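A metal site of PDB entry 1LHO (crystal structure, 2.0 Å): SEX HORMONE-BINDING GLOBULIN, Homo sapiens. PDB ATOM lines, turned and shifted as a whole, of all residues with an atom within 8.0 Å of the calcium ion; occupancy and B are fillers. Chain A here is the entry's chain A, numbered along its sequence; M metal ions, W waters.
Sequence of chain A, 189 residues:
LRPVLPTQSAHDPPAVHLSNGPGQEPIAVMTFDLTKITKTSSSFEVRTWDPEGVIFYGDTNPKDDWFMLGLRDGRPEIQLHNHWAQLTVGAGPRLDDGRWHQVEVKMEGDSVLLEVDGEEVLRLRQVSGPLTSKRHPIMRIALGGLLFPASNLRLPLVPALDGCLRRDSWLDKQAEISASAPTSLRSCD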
ATOM      1  N   SER A  19     -18.328  -8.110   5.769  1.00  0.00           N
ATOM      2  CA  SER A  19     -19.632  -7.489   5.667  1.00  0.00           C
ATOM      3  C   SER A  19     -19.996  -6.815   6.986  1.00  0.00           C
ATOM      4  O   SER A  19     -19.772  -7.372   8.066  1.00  0.00           O
ATOM      5  CB  SER A  19     -20.681  -8.545   5.316  1.00  0.00           C
ATOM      6  OG  SER A  19     -20.628  -9.638   6.216  1.00  0.00           O
ATOM      7  N   THR A  48     -14.953 -18.419   4.147  1.00  0.00           N
ATOM      8  CA  THR A  48     -16.386 -18.164   4.055  1.00  0.00           C
ATOM      9  C   THR A  48     -17.194 -19.389   3.634  1.00  0.00           C
ATOM     10  O   THR A  48     -16.644 -20.352   3.093  1.00  0.00           O
ATOM     11  CB  THR A  48     -16.649 -17.064   3.007  1.00  0.00           C
ATOM     12  OG1 THR A  48     -18.045 -16.789   2.905  1.00  0.00           O
ATOM     13  CG2 THR A  48     -16.134 -17.524   1.656  1.00  0.00           C
ATOM     14  N   TRP A  49     -18.504 -19.348   3.875  1.00  0.00           N
ATOM     15  CA  TRP A  49     -19.418 -20.404   3.472  1.00  0.00           C
ATOM     16  C   TRP A  49     -20.382 -19.764   2.472  1.00  0.00           C
ATOM     17  O   TRP A  49     -21.232 -20.432   1.912  1.00  0.00           O
ATOM     18  CB  TRP A  49     -20.238 -20.936   4.673  1.00  0.00           C
ATOM     19  CG  TRP A  49     -19.449 -21.661   5.717  1.00  0.00           C
ATOM     20  CD1 TRP A  49     -19.096 -21.196   6.954  1.00  0.00           C
ATOM     21  CD2 TRP A  49     -18.895 -22.990   5.611  1.00  0.00           C
ATOM     22  NE1 TRP A  49     -18.367 -22.151   7.631  1.00  0.00           N
ATOM     23  CE2 TRP A  49     -18.229 -23.253   6.829  1.00  0.00           C
ATOM     24  CE3 TRP A  49     -18.904 -23.970   4.611  1.00  0.00           C
ATOM     25  CZ2 TRP A  49     -17.564 -24.466   7.068  1.00  0.00           C
ATOM     26  CZ3 TRP A  49     -18.242 -25.177   4.858  1.00  0.00           C
ATOM     27  CH2 TRP A  49     -17.589 -25.408   6.076  1.00  0.00           C
ATOM     28  N   ASP A  50     -20.226 -18.458   2.244  1.00  0.00           N
ATOM     29  CA  ASP A  50     -21.066 -17.664   1.337  1.00  0.00           C
ATOM     30  C   ASP A  50     -20.685 -17.894  -0.128  1.00  0.00           C
ATOM     31  O   ASP A  50     -19.530 -17.644  -0.529  1.00  0.00           O
ATOM     32  CB  ASP A  50     -20.906 -16.185   1.689  1.00  0.00           C
ATOM     33  CG  ASP A  50     -22.026 -15.309   1.137  1.00  0.00           C
ATOM     34  OD1 ASP A  50     -22.762 -15.723   0.215  1.00  0.00           O
ATOM     35  OD2 ASP A  50     -22.146 -14.172   1.643  1.00  0.00           O
ATOM     36  N   PRO A  51     -21.632 -18.366  -0.952  1.00  0.00           N
ATOM     37  CA  PRO A  51     -21.348 -18.609  -2.368  1.00  0.00           C
ATOM     38  C   PRO A  51     -21.336 -17.380  -3.294  1.00  0.00           C
ATOM     39  O   PRO A  51     -20.856 -17.467  -4.422  1.00  0.00           O
ATOM     40  CB  PRO A  51     -22.449 -19.582  -2.776  1.00  0.00           C
ATOM     41  CG  PRO A  51     -23.628 -19.085  -1.952  1.00  0.00           C
ATOM     42  CD  PRO A  51     -22.984 -18.836  -0.592  1.00  0.00           C
ATOM     43  N   GLU A  52     -21.871 -16.264  -2.818  1.00  0.00           N
ATOM     44  CA  GLU A  52     -21.962 -15.065  -3.661  1.00  0.00           C
ATOM     45  C   GLU A  52     -21.616 -13.752  -2.960  1.00  0.00           C
ATOM     46  O   GLU A  52     -21.969 -13.559  -1.805  1.00  0.00           O
ATOM     47  CB  GLU A  52     -23.375 -14.953  -4.219  1.00  0.00           C
ATOM     48  CG  GLU A  52     -23.585 -13.768  -5.143  1.00  0.00           C
ATOM     49  CD  GLU A  52     -24.889 -13.850  -5.912  1.00  0.00           C
ATOM     50  OE1 GLU A  52     -25.151 -14.914  -6.530  1.00  0.00           O
ATOM     51  OE2 GLU A  52     -25.641 -12.856  -5.911  1.00  0.00           O
ATOM     52  N   GLY A  53     -20.947 -12.851  -3.658  1.00  0.00           N
ATOM     53  CA  GLY A  53     -20.597 -11.583  -3.038  1.00  0.00           C
ATOM     54  C   GLY A  53     -19.325 -10.956  -3.533  1.00  0.00           C
ATOM     55  O   GLY A  53     -18.587 -11.550  -4.335  1.00  0.00           O
ATOM     56  N   VAL A  54     -19.045  -9.758  -3.041  1.00  0.00           N
ATOM     57  CA  VAL A  54     -17.861  -9.016  -3.441  1.00  0.00           C
ATOM     58  C   VAL A  54     -16.741  -9.133  -2.428  1.00  0.00           C
ATOM     59  O   VAL A  54     -16.937  -8.854  -1.236  1.00  0.00           O
ATOM     60  CB  VAL A  54     -18.169  -7.507  -3.583  1.00  0.00           C
ATOM     61  CG1 VAL A  54     -16.864  -6.754  -3.925  1.00  0.00           C
ATOM     62  CG2 VAL A  54     -19.245  -7.284  -4.634  1.00  0.00           C
ATOM     63  N   LEU A  71     -17.329 -13.648  -5.673  1.00  0.00           N
ATOM     64  CA  LEU A  71     -17.631 -15.061  -5.796  1.00  0.00           C
ATOM     65  C   LEU A  71     -19.045 -15.176  -6.361  1.00  0.00           C
ATOM     66  O   LEU A  71     -19.900 -14.321  -6.077  1.00  0.00           O
ATOM     67  CB  LEU A  71     -17.615 -15.764  -4.440  1.00  0.00           C
ATOM     68  CG  LEU A  71     -16.323 -15.867  -3.635  1.00  0.00           C
ATOM     69  CD1 LEU A  71     -16.651 -16.552  -2.309  1.00  0.00           C
ATOM     70  CD2 LEU A  71     -15.248 -16.640  -4.409  1.00  0.00           C
ATOM     71  N   LEU A 157     -24.970  -9.139  -8.930  1.00  0.00           N
ATOM     72  CA  LEU A 157     -24.917 -10.176  -7.919  1.00  0.00           C
ATOM     73  C   LEU A 157     -25.222  -9.404  -6.639  1.00  0.00           C
ATOM     74  O   LEU A 157     -25.207  -8.162  -6.655  1.00  0.00           O
ATOM     75  CB  LEU A 157     -23.542 -10.833  -7.831  1.00  0.00           C
ATOM     76  CG  LEU A 157     -22.261  -9.960  -7.790  1.00  0.00           C
ATOM     77  CD1 LEU A 157     -22.239  -9.083  -6.515  1.00  0.00           C
ATOM     78  CD2 LEU A 157     -21.045 -10.885  -7.825  1.00  0.00           C
ATOM     79  N   VAL A 158     -25.535 -10.106  -5.554  1.00  0.00           N
ATOM     80  CA  VAL A 158     -25.807  -9.463  -4.270  1.00  0.00           C
ATOM     81  C   VAL A 158     -24.420  -9.375  -3.624  1.00  0.00           C
ATOM     82  O   VAL A 158     -23.827 -10.390  -3.275  1.00  0.00           O
ATOM     83  CB  VAL A 158     -26.786 -10.303  -3.422  1.00  0.00           C
ATOM     84  CG1 VAL A 158     -27.044  -9.622  -2.095  1.00  0.00           C
ATOM     85  CG2 VAL A 158     -28.099 -10.491  -4.189  1.00  0.00           C
ATOM     86  N   PRO A 159     -23.903  -8.146  -3.437  1.00  0.00           N
ATOM     87  CA  PRO A 159     -22.574  -7.859  -2.860  1.00  0.00           C
ATOM     88  C   PRO A 159     -22.177  -8.339  -1.465  1.00  0.00           C
ATOM     89  O   PRO A 159     -20.999  -8.588  -1.219  1.00  0.00           O
ATOM     90  CB  PRO A 159     -22.465  -6.332  -2.995  1.00  0.00           C
ATOM     91  CG  PRO A 159     -23.877  -5.884  -2.855  1.00  0.00           C
ATOM     92  CD  PRO A 159     -24.657  -6.902  -3.677  1.00  0.00           C
ATOM     93  N   ALA A 160     -23.144  -8.479  -0.555  1.00  0.00           N
ATOM     94  CA  ALA A 160     -22.822  -8.929   0.796  1.00  0.00           C
ATOM     95  C   ALA A 160     -22.055 -10.261   0.789  1.00  0.00           C
ATOM     96  O   ALA A 160     -22.535 -11.270   0.284  1.00  0.00           O
ATOM     97  CB  ALA A 160     -24.128  -9.077   1.621  1.00  0.00           C
ATOM     98  N   LEU A 161     -20.853 -10.239   1.352  1.00  0.00           N
ATOM     99  CA  LEU A 161     -20.042 -11.457   1.423  1.00  0.00           C
ATOM    100  C   LEU A 161     -19.770 -11.786   2.892  1.00  0.00           C
ATOM    101  O   LEU A 161     -18.926 -11.170   3.542  1.00  0.00           O
ATOM    102  CB  LEU A 161     -18.717 -11.266   0.665  1.00  0.00           C
ATOM    103  CG  LEU A 161     -17.988 -12.523   0.146  1.00  0.00           C
ATOM    104  CD1 LEU A 161     -17.254 -13.237   1.286  1.00  0.00           C
ATOM    105  CD2 LEU A 161     -18.986 -13.465  -0.515  1.00  0.00           C
ATOM    106  N   ASP A 162     -20.527 -12.754   3.405  1.00  0.00           N
ATOM    107  CA  ASP A 162     -20.373 -13.175   4.792  1.00  0.00           C
ATOM    108  C   ASP A 162     -19.126 -14.024   4.930  1.00  0.00           C
ATOM    109  O   ASP A 162     -19.181 -15.251   4.812  1.00  0.00           O
ATOM    110  CB  ASP A 162     -21.592 -13.995   5.228  1.00  0.00           C
ATOM    111  CG  ASP A 162     -21.725 -14.070   6.734  1.00  0.00           C
ATOM    112  OD1 ASP A 162     -20.685 -14.121   7.421  1.00  0.00           O
ATOM    113  OD2 ASP A 162     -22.871 -14.074   7.217  1.00  0.00           O
ATOM    114  N   GLY A 163     -18.008 -13.370   5.197  1.00  0.00           N
ATOM    115  CA  GLY A 163     -16.748 -14.072   5.334  1.00  0.00           C
ATOM    116  C   GLY A 163     -15.710 -13.266   6.091  1.00  0.00           C
ATOM    117  O   GLY A 163     -15.964 -12.134   6.518  1.00  0.00           O
HETATM  118 CA    CA M   1     -23.536 -13.419   0.012  1.00  0.00          CA
HETATM  119  O   HOH W   1     -25.225 -15.014  -0.797  1.00  0.00           O
HETATM  120  O   HOH W   2     -24.798 -12.197  -1.351  1.00  0.00           O
HETATM  121  O   HOH W   3     -25.149 -12.996   1.847  1.00  0.00           O
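The calcium ion is bound by water W2, the side-chain carboxylate (OD2) of Asp 50, the backbone carbonyl oxygen (O) of Ala 160, the backbone carbonyl oxygen (O) of Glu 52, the side-chain carboxylate (OD1) of Asp 50, water W1 and water W3.
The backbone NH (N) of Asp 50 lies within hydrogen-bond range of the side-chain hydroxyl (OG1) of Thr 48, 2.8 Å away. OE2 of Glu 52 is in hydrogen-bond range of N of Val 158, at 2.8 Å. The side-chain carboxylate of Asp 50 lies close to the backbone NH of Asp 162, at 2.8 Å.
Three residues have an atom within 4 Å of the calcium ion: Asp 50, Glu 52 and Ala 160. Along chain A the residues within 4 Å of the calcium ion span positions 50 to 160.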
